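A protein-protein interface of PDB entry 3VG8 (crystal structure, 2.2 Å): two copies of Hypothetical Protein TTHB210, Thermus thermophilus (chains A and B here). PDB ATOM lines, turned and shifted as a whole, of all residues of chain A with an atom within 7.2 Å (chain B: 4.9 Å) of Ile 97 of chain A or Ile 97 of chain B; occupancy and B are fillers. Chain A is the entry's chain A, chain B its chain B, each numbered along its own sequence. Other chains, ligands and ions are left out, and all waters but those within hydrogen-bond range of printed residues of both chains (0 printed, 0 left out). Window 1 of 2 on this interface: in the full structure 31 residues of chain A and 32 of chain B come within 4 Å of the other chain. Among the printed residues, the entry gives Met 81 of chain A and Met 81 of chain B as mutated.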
ATOM      1  N   GLU A  30      15.973  12.728  22.440  1.00  0.00           N
ATOM      2  CA  GLU A  30      15.606  13.965  23.111  1.00  0.00           C
ATOM      3  C   GLU A  30      16.133  14.150  24.535  1.00  0.00           C
ATOM      4  O   GLU A  30      16.461  15.275  24.936  1.00  0.00           O
ATOM      5  CB  GLU A  30      14.079  14.127  23.148  1.00  0.00           C
ATOM      6  CG  GLU A  30      13.407  14.230  21.790  1.00  0.00           C
ATOM      7  CD  GLU A  30      13.162  12.868  21.163  1.00  0.00           C
ATOM      8  OE1 GLU A  30      12.674  12.812  20.020  1.00  0.00           O
ATOM      9  OE2 GLU A  30      13.460  11.850  21.815  1.00  0.00           O
ATOM     10  N   PRO A  32      15.514  14.644  28.326  1.00  0.00           N
ATOM     11  CA  PRO A  32      16.525  15.696  28.229  1.00  0.00           C
ATOM     12  C   PRO A  32      17.861  15.380  28.874  1.00  0.00           C
ATOM     13  O   PRO A  32      17.959  14.482  29.707  1.00  0.00           O
ATOM     14  CB  PRO A  32      15.845  16.875  28.920  1.00  0.00           C
ATOM     15  CG  PRO A  32      15.132  16.188  30.057  1.00  0.00           C
ATOM     16  CD  PRO A  32      14.515  14.978  29.365  1.00  0.00           C
ATOM     17  N   PHE A  33      18.870  16.165  28.480  1.00  0.00           N
ATOM     18  CA  PHE A  33      20.250  16.093  28.975  1.00  0.00           C
ATOM     19  C   PHE A  33      20.445  17.134  30.082  1.00  0.00           C
ATOM     20  O   PHE A  33      19.834  18.207  30.056  1.00  0.00           O
ATOM     21  CB  PHE A  33      21.271  16.474  27.888  1.00  0.00           C
ATOM     22  CG  PHE A  33      21.470  15.451  26.800  1.00  0.00           C
ATOM     23  CD1 PHE A  33      20.554  15.311  25.773  1.00  0.00           C
ATOM     24  CD2 PHE A  33      22.637  14.691  26.756  1.00  0.00           C
ATOM     25  CE1 PHE A  33      20.799  14.440  24.714  1.00  0.00           C
ATOM     26  CE2 PHE A  33      22.888  13.816  25.696  1.00  0.00           C
ATOM     27  CZ  PHE A  33      21.968  13.694  24.671  1.00  0.00           C
ATOM     28  N   VAL A  45      18.903  22.360  31.515  1.00  0.00           N
ATOM     29  CA  VAL A  45      18.275  21.104  31.124  1.00  0.00           C
ATOM     30  C   VAL A  45      18.162  21.293  29.609  1.00  0.00           C
ATOM     31  O   VAL A  45      17.730  22.338  29.141  1.00  0.00           O
ATOM     32  CB  VAL A  45      16.879  20.929  31.781  1.00  0.00           C
ATOM     33  CG1 VAL A  45      16.208  19.660  31.276  1.00  0.00           C
ATOM     34  CG2 VAL A  45      17.033  20.831  33.297  1.00  0.00           C
ATOM     35  N   VAL A  46      18.591  20.300  28.846  1.00  0.00           N
ATOM     36  CA  VAL A  46      18.581  20.412  27.398  1.00  0.00           C
ATOM     37  C   VAL A  46      17.842  19.274  26.694  1.00  0.00           C
ATOM     38  O   VAL A  46      18.232  18.110  26.793  1.00  0.00           O
ATOM     39  CB  VAL A  46      20.034  20.412  26.818  1.00  0.00           C
ATOM     40  CG1 VAL A  46      19.984  20.529  25.300  1.00  0.00           C
ATOM     41  CG2 VAL A  46      20.862  21.568  27.395  1.00  0.00           C
ATOM     42  N   PHE A  47      16.779  19.617  25.985  1.00  0.00           N
ATOM     43  CA  PHE A  47      16.060  18.627  25.198  1.00  0.00           C
ATOM     44  C   PHE A  47      16.747  18.691  23.817  1.00  0.00           C
ATOM     45  O   PHE A  47      16.953  19.773  23.274  1.00  0.00           O
ATOM     46  CB  PHE A  47      14.588  19.003  25.065  1.00  0.00           C
ATOM     47  CG  PHE A  47      13.811  18.932  26.362  1.00  0.00           C
ATOM     48  CD1 PHE A  47      13.801  20.000  27.243  1.00  0.00           C
ATOM     49  CD2 PHE A  47      13.066  17.791  26.686  1.00  0.00           C
ATOM     50  CE1 PHE A  47      13.062  19.942  28.427  1.00  0.00           C
ATOM     51  CE2 PHE A  47      12.329  17.724  27.865  1.00  0.00           C
ATOM     52  CZ  PHE A  47      12.329  18.807  28.738  1.00  0.00           C
ATOM     53  N   MET A  48      17.105  17.532  23.274  1.00  0.00           N
ATOM     54  CA  MET A  48      17.777  17.401  21.978  1.00  0.00           C
ATOM     55  C   MET A  48      16.760  16.938  20.965  1.00  0.00           C
ATOM     56  O   MET A  48      16.617  15.735  20.724  1.00  0.00           O
ATOM     57  CB  MET A  48      18.859  16.340  22.092  1.00  0.00           C
ATOM     58  CG  MET A  48      20.116  16.838  22.735  1.00  0.00           C
ATOM     59  SD  MET A  48      21.184  17.460  21.306  1.00  0.00           S
ATOM     60  CE  MET A  48      21.508  15.722  20.522  1.00  0.00           C
ATOM     61  N   VAL A  49      16.072  17.886  20.354  1.00  0.00           N
ATOM     62  CA  VAL A  49      15.009  17.561  19.424  1.00  0.00           C
ATOM     63  C   VAL A  49      15.408  17.450  17.954  1.00  0.00           C
ATOM     64  O   VAL A  49      15.861  18.427  17.345  1.00  0.00           O
ATOM     65  CB  VAL A  49      13.875  18.606  19.562  1.00  0.00           C
ATOM     66  CG1 VAL A  49      12.608  18.117  18.859  1.00  0.00           C
ATOM     67  CG2 VAL A  49      13.606  18.882  21.044  1.00  0.00           C
ATOM     68  N   LEU A  54      10.097  17.448  14.224  1.00  0.00           N
ATOM     69  CA  LEU A  54       9.352  18.705  14.172  1.00  0.00           C
ATOM     70  C   LEU A  54       8.740  18.918  12.785  1.00  0.00           C
ATOM     71  O   LEU A  54       7.619  19.425  12.660  1.00  0.00           O
ATOM     72  CB  LEU A  54      10.257  19.889  14.549  1.00  0.00           C
ATOM     73  CG  LEU A  54      10.859  19.920  15.967  1.00  0.00           C
ATOM     74  CD1 LEU A  54      11.655  21.199  16.162  1.00  0.00           C
ATOM     75  CD2 LEU A  54       9.749  19.833  17.020  1.00  0.00           C
ATOM     76  N   VAL A  79      15.277  30.709  28.458  1.00  0.00           N
ATOM     77  CA  VAL A  79      15.263  29.577  27.555  1.00  0.00           C
ATOM     78  C   VAL A  79      16.119  29.874  26.315  1.00  0.00           C
ATOM     79  O   VAL A  79      16.219  31.026  25.872  1.00  0.00           O
ATOM     80  CB  VAL A  79      13.826  29.291  27.075  1.00  0.00           C
ATOM     81  CG1 VAL A  79      13.850  28.389  25.852  1.00  0.00           C
ATOM     82  CG2 VAL A  79      13.029  28.676  28.186  1.00  0.00           C
ATOM     83  N   ASN A  80      16.761  28.850  25.773  1.00  0.00           N
ATOM     84  CA  ASN A  80      17.486  29.013  24.518  1.00  0.00           C
ATOM     85  C   ASN A  80      16.896  27.960  23.592  1.00  0.00           C
ATOM     86  O   ASN A  80      16.419  26.921  24.055  1.00  0.00           O
ATOM     87  CB  ASN A  80      18.985  28.685  24.610  1.00  0.00           C
ATOM     88  CG  ASN A  80      19.758  29.652  25.469  1.00  0.00           C
ATOM     89  OD1 ASN A  80      19.469  30.847  25.494  1.00  0.00           O
ATOM     90  ND2 ASN A  80      20.776  29.138  26.164  1.00  0.00           N
ATOM     91  N   MET A  81      16.943  28.228  22.291  1.00  0.00           N
ATOM     92  CA  MET A  81      16.517  27.287  21.270  1.00  0.00           C
ATOM     93  C   MET A  81      17.585  27.500  20.213  1.00  0.00           C
ATOM     94  O   MET A  81      17.538  28.442  19.420  1.00  0.00           O
ATOM     95  CB  MET A  81      15.120  27.610  20.756  1.00  0.00           C
ATOM     96  CG  MET A  81      14.074  27.345  21.808  1.00  0.00           C
ATOM     97  SD  MET A  81      12.286  27.671  21.204  1.00  0.00           S
ATOM     98  CE  MET A  81      11.995  29.296  22.194  1.00  0.00           C
ATOM     99  N   ILE A  82      18.559  26.607  20.255  1.00  0.00           N
ATOM    100  CA  ILE A  82      19.743  26.638  19.411  1.00  0.00           C
ATOM    101  C   ILE A  82      19.926  25.421  18.518  1.00  0.00           C
ATOM    102  O   ILE A  82      19.789  24.271  18.959  1.00  0.00           O
ATOM    103  CB  ILE A  82      21.007  26.705  20.289  1.00  0.00           C
ATOM    104  CG1 ILE A  82      20.889  27.847  21.295  1.00  0.00           C
ATOM    105  CG2 ILE A  82      22.235  26.881  19.426  1.00  0.00           C
ATOM    106  CD1 ILE A  82      21.969  27.797  22.387  1.00  0.00           C
ATOM    107  N   HIS A  94      19.463  18.787  14.876  1.00  0.00           N
ATOM    108  CA  HIS A  94      18.650  18.805  16.091  1.00  0.00           C
ATOM    109  C   HIS A  94      18.587  20.227  16.588  1.00  0.00           C
ATOM    110  O   HIS A  94      19.377  21.082  16.199  1.00  0.00           O
ATOM    111  CB  HIS A  94      19.268  17.965  17.229  1.00  0.00           C
ATOM    112  CG  HIS A  94      19.320  16.497  16.945  1.00  0.00           C
ATOM    113  ND1 HIS A  94      20.087  15.962  15.930  1.00  0.00           N
ATOM    114  CD2 HIS A  94      18.664  15.455  17.511  1.00  0.00           C
ATOM    115  CE1 HIS A  94      19.898  14.656  15.878  1.00  0.00           C
ATOM    116  NE2 HIS A  94      19.037  14.322  16.825  1.00  0.00           N
ATOM    117  N   TYR A  95      17.630  20.483  17.455  1.00  0.00           N
ATOM    118  CA  TYR A  95      17.547  21.783  18.077  1.00  0.00           C
ATOM    119  C   TYR A  95      17.741  21.509  19.566  1.00  0.00           C
ATOM    120  O   TYR A  95      17.247  20.506  20.092  1.00  0.00           O
ATOM    121  CB  TYR A  95      16.185  22.435  17.812  1.00  0.00           C
ATOM    122  CG  TYR A  95      16.339  23.692  17.010  1.00  0.00           C
ATOM    123  CD1 TYR A  95      16.487  24.927  17.643  1.00  0.00           C
ATOM    124  CD2 TYR A  95      16.489  23.638  15.618  1.00  0.00           C
ATOM    125  CE1 TYR A  95      16.794  26.076  16.914  1.00  0.00           C
ATOM    126  CE2 TYR A  95      16.801  24.789  14.879  1.00  0.00           C
ATOM    127  CZ  TYR A  95      16.952  25.998  15.535  1.00  0.00           C
ATOM    128  OH  TYR A  95      17.243  27.141  14.829  1.00  0.00           O
ATOM    129  N   HIS A  96      18.490  22.378  20.228  1.00  0.00           N
ATOM    130  CA  HIS A  96      18.712  22.260  21.657  1.00  0.00           C
ATOM    131  C   HIS A  96      17.720  23.195  22.331  1.00  0.00           C
ATOM    132  O   HIS A  96      17.896  24.414  22.284  1.00  0.00           O
ATOM    133  CB  HIS A  96      20.130  22.704  22.046  1.00  0.00           C
ATOM    134  CG  HIS A  96      21.206  21.775  21.585  1.00  0.00           C
ATOM    135  ND1 HIS A  96      22.527  21.926  21.954  1.00  0.00           N
ATOM    136  CD2 HIS A  96      21.162  20.689  20.778  1.00  0.00           C
ATOM    137  CE1 HIS A  96      23.248  20.972  21.394  1.00  0.00           C
ATOM    138  NE2 HIS A  96      22.444  20.208  20.676  1.00  0.00           N
ATOM    139  N   ILE A  97      16.674  22.635  22.928  1.00  0.00           N
ATOM    140  CA  ILE A  97      15.695  23.454  23.633  1.00  0.00           C
ATOM    141  C   ILE A  97      16.229  23.432  25.050  1.00  0.00           C
ATOM    142  O   ILE A  97      16.250  22.397  25.721  1.00  0.00           O
ATOM    143  CB  ILE A  97      14.278  22.855  23.521  1.00  0.00           C
ATOM    144  CG1 ILE A  97      13.927  22.639  22.047  1.00  0.00           C
ATOM    145  CG2 ILE A  97      13.268  23.795  24.086  1.00  0.00           C
ATOM    146  CD1 ILE A  97      14.093  23.902  21.177  1.00  0.00           C
ATOM    147  N   GLU A  98      16.687  24.585  25.495  1.00  0.00           N
ATOM    148  CA  GLU A  98      17.330  24.681  26.781  1.00  0.00           C
ATOM    149  C   GLU A  98      16.624  25.496  27.842  1.00  0.00           C
ATOM    150  O   GLU A  98      16.188  26.608  27.582  1.00  0.00           O
ATOM    151  CB  GLU A  98      18.746  25.252  26.572  1.00  0.00           C
ATOM    152  CG  GLU A  98      19.537  24.567  25.444  1.00  0.00           C
ATOM    153  CD  GLU A  98      20.982  25.065  25.294  1.00  0.00           C
ATOM    154  OE1 GLU A  98      21.821  24.278  24.805  1.00  0.00           O
ATOM    155  OE2 GLU A  98      21.276  26.229  25.644  1.00  0.00           O
ATOM    156  N   LEU A  99      16.515  24.930  29.042  1.00  0.00           N
ATOM    157  CA  LEU A  99      15.918  25.649  30.170  1.00  0.00           C
ATOM    158  C   LEU A  99      17.164  25.909  31.030  1.00  0.00           C
ATOM    159  O   LEU A  99      17.703  24.994  31.643  1.00  0.00           O
ATOM    160  CB  LEU A  99      14.906  24.778  30.924  1.00  0.00           C
ATOM    161  CG  LEU A  99      13.897  23.944  30.127  1.00  0.00           C
ATOM    162  CD1 LEU A  99      12.784  23.491  31.062  1.00  0.00           C
ATOM    163  CD2 LEU A  99      13.320  24.742  28.981  1.00  0.00           C
ATOM    164  N   VAL A 100      17.627  27.158  31.019  1.00  0.00           N
ATOM    165  CA  VAL A 100      18.834  27.574  31.724  1.00  0.00           C
ATOM    166  C   VAL A 100      18.534  28.114  33.115  1.00  0.00           C
ATOM    167  O   VAL A 100      17.660  28.961  33.290  1.00  0.00           O
ATOM    168  CB  VAL A 100      19.564  28.647  30.903  1.00  0.00           C
ATOM    169  CG1 VAL A 100      20.954  28.902  31.476  1.00  0.00           C
ATOM    170  CG2 VAL A 100      19.638  28.200  29.443  1.00  0.00           C
ATOM    171  N   VAL B  45       3.799  28.217  30.655  1.00  0.00           N
ATOM    172  CA  VAL B  45       4.535  29.266  29.966  1.00  0.00           C
ATOM    173  C   VAL B  45       4.751  28.766  28.530  1.00  0.00           C
ATOM    174  O   VAL B  45       5.404  27.738  28.309  1.00  0.00           O
ATOM    175  CB  VAL B  45       5.879  29.461  30.675  1.00  0.00           C
ATOM    176  CG1 VAL B  45       6.704  30.513  29.978  1.00  0.00           C
ATOM    177  CG2 VAL B  45       5.615  29.850  32.118  1.00  0.00           C
ATOM    178  N   VAL B  46       4.211  29.491  27.554  1.00  0.00           N
ATOM    179  CA  VAL B  46       4.275  29.049  26.162  1.00  0.00           C
ATOM    180  C   VAL B  46       5.086  29.921  25.186  1.00  0.00           C
ATOM    181  O   VAL B  46       4.760  31.082  24.985  1.00  0.00           O
ATOM    182  CB  VAL B  46       2.833  28.911  25.604  1.00  0.00           C
ATOM    183  CG1 VAL B  46       2.850  28.360  24.190  1.00  0.00           C
ATOM    184  CG2 VAL B  46       2.006  28.016  26.506  1.00  0.00           C
ATOM    185  N   PHE B  47       6.141  29.357  24.601  1.00  0.00           N
ATOM    186  CA  PHE B  47       6.948  30.068  23.602  1.00  0.00           C
ATOM    187  C   PHE B  47       6.426  29.679  22.217  1.00  0.00           C
ATOM    188  O   PHE B  47       6.146  28.511  21.960  1.00  0.00           O
ATOM    189  CB  PHE B  47       8.428  29.674  23.697  1.00  0.00           C
ATOM    190  CG  PHE B  47       9.071  30.087  24.972  1.00  0.00           C
ATOM    191  CD1 PHE B  47       9.027  29.263  26.086  1.00  0.00           C
ATOM    192  CD2 PHE B  47       9.664  31.342  25.088  1.00  0.00           C
ATOM    193  CE1 PHE B  47       9.559  29.684  27.294  1.00  0.00           C
ATOM    194  CE2 PHE B  47      10.196  31.765  26.291  1.00  0.00           C
ATOM    195  CZ  PHE B  47      10.143  30.934  27.394  1.00  0.00           C
ATOM    196  N   VAL B  49       7.218  29.483  18.207  1.00  0.00           N
ATOM    197  CA  VAL B  49       8.286  29.546  17.211  1.00  0.00           C
ATOM    198  C   VAL B  49       7.868  29.001  15.853  1.00  0.00           C
ATOM    199  O   VAL B  49       7.274  27.921  15.755  1.00  0.00           O
ATOM    200  CB  VAL B  49       9.586  28.797  17.662  1.00  0.00           C
ATOM    201  CG1 VAL B  49      10.121  29.419  18.945  1.00  0.00           C
ATOM    202  CG2 VAL B  49       9.322  27.324  17.848  1.00  0.00           C
ATOM    203  N   VAL B  79       7.452  19.328  29.947  1.00  0.00           N
ATOM    204  CA  VAL B  79       7.487  20.140  28.744  1.00  0.00           C
ATOM    205  C   VAL B  79       6.653  19.515  27.628  1.00  0.00           C
ATOM    206  O   VAL B  79       6.549  18.299  27.528  1.00  0.00           O
ATOM    207  CB  VAL B  79       8.954  20.314  28.256  1.00  0.00           C
ATOM    208  CG1 VAL B  79       8.997  20.941  26.866  1.00  0.00           C
ATOM    209  CG2 VAL B  79       9.705  21.181  29.235  1.00  0.00           C
ATOM    210  N   ASN B  80       6.023  20.359  26.819  1.00  0.00           N
ATOM    211  CA  ASN B  80       5.267  19.879  25.670  1.00  0.00           C
ATOM    212  C   ASN B  80       5.802  20.675  24.496  1.00  0.00           C
ATOM    213  O   ASN B  80       6.237  21.820  24.667  1.00  0.00           O
ATOM    214  CB  ASN B  80       3.764  20.223  25.725  1.00  0.00           C
ATOM    215  CG  ASN B  80       3.027  19.577  26.873  1.00  0.00           C
ATOM    216  OD1 ASN B  80       3.313  18.446  27.295  1.00  0.00           O
ATOM    217  ND2 ASN B  80       2.034  20.295  27.371  1.00  0.00           N
ATOM    218  N   MET B  81       5.724  20.092  23.308  1.00  0.00           N
ATOM    219  CA  MET B  81       6.100  20.788  22.086  1.00  0.00           C
ATOM    220  C   MET B  81       5.005  20.351  21.140  1.00  0.00           C
ATOM    221  O   MET B  81       5.023  19.227  20.649  1.00  0.00           O
ATOM    222  CB  MET B  81       7.478  20.343  21.600  1.00  0.00           C
ATOM    223  CG  MET B  81       8.578  20.759  22.558  1.00  0.00           C
ATOM    224  SD  MET B  81      10.333  20.265  21.881  1.00  0.00           S
ATOM    225  CE  MET B  81      11.224  19.929  23.565  1.00  0.00           C
ATOM    226  N   TYR B  95       5.480  25.979  16.388  1.00  0.00           N
ATOM    227  CA  TYR B  95       5.577  25.018  17.468  1.00  0.00           C
ATOM    228  C   TYR B  95       5.367  25.815  18.750  1.00  0.00           C
ATOM    229  O   TYR B  95       5.811  26.976  18.879  1.00  0.00           O
ATOM    230  CB  TYR B  95       6.923  24.281  17.484  1.00  0.00           C
ATOM    231  CG  TYR B  95       6.790  22.839  17.035  1.00  0.00           C
ATOM    232  CD1 TYR B  95       6.444  21.820  17.939  1.00  0.00           C
ATOM    233  CD2 TYR B  95       6.928  22.504  15.688  1.00  0.00           C
ATOM    234  CE1 TYR B  95       6.238  20.497  17.493  1.00  0.00           C
ATOM    235  CE2 TYR B  95       6.729  21.220  15.241  1.00  0.00           C
ATOM    236  CZ  TYR B  95       6.382  20.213  16.142  1.00  0.00           C
ATOM    237  OH  TYR B  95       6.165  18.940  15.652  1.00  0.00           O
ATOM    238  N   HIS B  96       4.606  25.223  19.658  1.00  0.00           N
ATOM    239  CA  HIS B  96       4.343  25.843  20.940  1.00  0.00           C
ATOM    240  C   HIS B  96       5.255  25.101  21.883  1.00  0.00           C
ATOM    241  O   HIS B  96       5.113  23.903  22.047  1.00  0.00           O
ATOM    242  CB  HIS B  96       2.890  25.615  21.384  1.00  0.00           C
ATOM    243  CG  HIS B  96       1.885  26.450  20.657  1.00  0.00           C
ATOM    244  ND1 HIS B  96       1.816  26.512  19.281  1.00  0.00           N
ATOM    245  CD2 HIS B  96       0.871  27.223  21.118  1.00  0.00           C
ATOM    246  CE1 HIS B  96       0.804  27.285  18.926  1.00  0.00           C
ATOM    247  NE2 HIS B  96       0.216  27.729  20.022  1.00  0.00           N
ATOM    248  N   ILE B  97       6.205  25.790  22.491  1.00  0.00           N
ATOM    249  CA  ILE B  97       7.082  25.120  23.427  1.00  0.00           C
ATOM    250  C   ILE B  97       6.529  25.543  24.781  1.00  0.00           C
ATOM    251  O   ILE B  97       6.554  26.721  25.157  1.00  0.00           O
ATOM    252  CB  ILE B  97       8.540  25.572  23.257  1.00  0.00           C
ATOM    253  CG1 ILE B  97       8.951  25.467  21.783  1.00  0.00           C
ATOM    254  CG2 ILE B  97       9.439  24.697  24.088  1.00  0.00           C
ATOM    255  CD1 ILE B  97       8.914  24.062  21.244  1.00  0.00           C
ATOM    256  N   GLU B  98       6.026  24.562  25.507  1.00  0.00           N
ATOM    257  CA  GLU B  98       5.380  24.815  26.772  1.00  0.00           C
ATOM    258  C   GLU B  98       6.099  24.277  28.010  1.00  0.00           C
ATOM    259  O   GLU B  98       6.509  23.116  28.059  1.00  0.00           O
ATOM    260  CB  GLU B  98       3.955  24.233  26.719  1.00  0.00           C
ATOM    261  CG  GLU B  98       3.289  24.266  25.341  1.00  0.00           C
ATOM    262  CD  GLU B  98       1.788  23.957  25.400  1.00  0.00           C
ATOM    263  OE1 GLU B  98       1.394  22.961  26.046  1.00  0.00           O
ATOM    264  OE2 GLU B  98       1.003  24.719  24.793  1.00  0.00           O
ATOM    265  N   LEU B  99       6.246  25.154  28.994  1.00  0.00           N
ATOM    266  CA  LEU B  99       6.838  24.818  30.286  1.00  0.00           C
ATOM    267  C   LEU B  99       5.605  24.716  31.193  1.00  0.00           C
ATOM    268  O   LEU B  99       5.018  25.732  31.552  1.00  0.00           O
ATOM    269  CB  LEU B  99       7.763  25.947  30.752  1.00  0.00           C
ATOM    270  CG  LEU B  99       9.208  25.863  30.247  1.00  0.00           C
ATOM    271  CD1 LEU B  99       9.219  25.819  28.734  1.00  0.00           C
ATOM    272  CD2 LEU B  99      10.019  27.051  30.770  1.00  0.00           C
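Phe 47 of chain A touches Val 79 of chain B, and with the chains exchanged Val 79 of chain A touches Phe 47 of chain B. Phe 47 of chain A touches Met 81 of chain B, and with the chains exchanged Met 81 of chain A touches Phe 47 of chain B. Val 49 of chain A touches Met 81 of chain B, and with the chains exchanged Met 81 of chain A touches Val 49 of chain B. Ile 97 of chain B touches its own counterpart, Ile 97 of chain A. Of the 8 pairs that touch across the chains among the printed residues, 7 have their exchanged pair printed and touching as well.
The backbone carbonyl oxygen (O) of Ile 97 of chain A sits at hydrogen-bond distance from the backbone NH (N) of Phe 47 of chain A (2.8 Å). The backbone NH of Tyr 95 of chain A lies within hydrogen-bond range of the backbone carbonyl oxygen of Val 49 of chain A, at 2.7 Å. The backbone carbonyl oxygen of Ile 97 of chain B is in hydrogen-bond range of the backbone NH of Phe 47 of chain B, at 2.7 Å. O of Val 49 of chain B lies within hydrogen-bond range of N of Tyr 95 of chain B (2.7 Å).
The side-chain hydroxyl (OH) of Tyr 95 of chain B lies close to the backbone carbonyl oxygen (O) of Leu 54 of chain A (3.4 Å).
Among the printed residues, pairs that only touch across the chains: Phe 47 of chain A with Val 79 of chain B (3.6 Å), Met 81 of chain A with Val 49 of chain B (3.6 Å), Val 49 of chain A with Met 81 of chain B (3.6 Å), Val 79 of chain A with Phe 47 of chain B (3.7 Å), Phe 47 of chain A with Met 81 of chain B (3.8 Å), Met 81 of chain A with Phe 47 of chain B (3.9 Å) and Ile 97 of chain A with Ile 97 of chain B (3.9 Å).
Of the printed residues of chain B, Met 81 of chain A touches Phe 47 (3.9 Å) and Val 49 (3.6 Å). Val 45 of chain B touches none of the printed residues of chain A. Of the printed residues of chain A, Phe 47 of chain B touches Val 79 (3.7 Å) and Met 81 (3.9 Å). Printed residues of chain A within 4 Å of Val 49 of chain B: Met 81 (3.6 Å). Printed residues of chain A within 4 Å of Met 81 of chain B: Phe 47 and Val 49. Printed residues of chain A within 4 Å of Tyr 95 of chain B: Leu 54. Of chain A, only Ile 97 (3.9 Å) comes within 4 Å of Ile 97 of chain B. The nearest printed residue of chain B that does not touch Val 79 of chain A is Leu 99 of chain B (4.3 Å).
Of the 20 printed residues of chain A, 6 touch a printed residue of chain B. Hydrophobic or aromatic side chains of chain A that line the printed part of chain B: Phe 47, Val 49, Leu 54, Val 79, Met 81 and Ile 97. Among the printed residues, no Asp or Glu carboxylate lies within 4 Å of a Lys or Arg side-chain nitrogen of the other chain.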
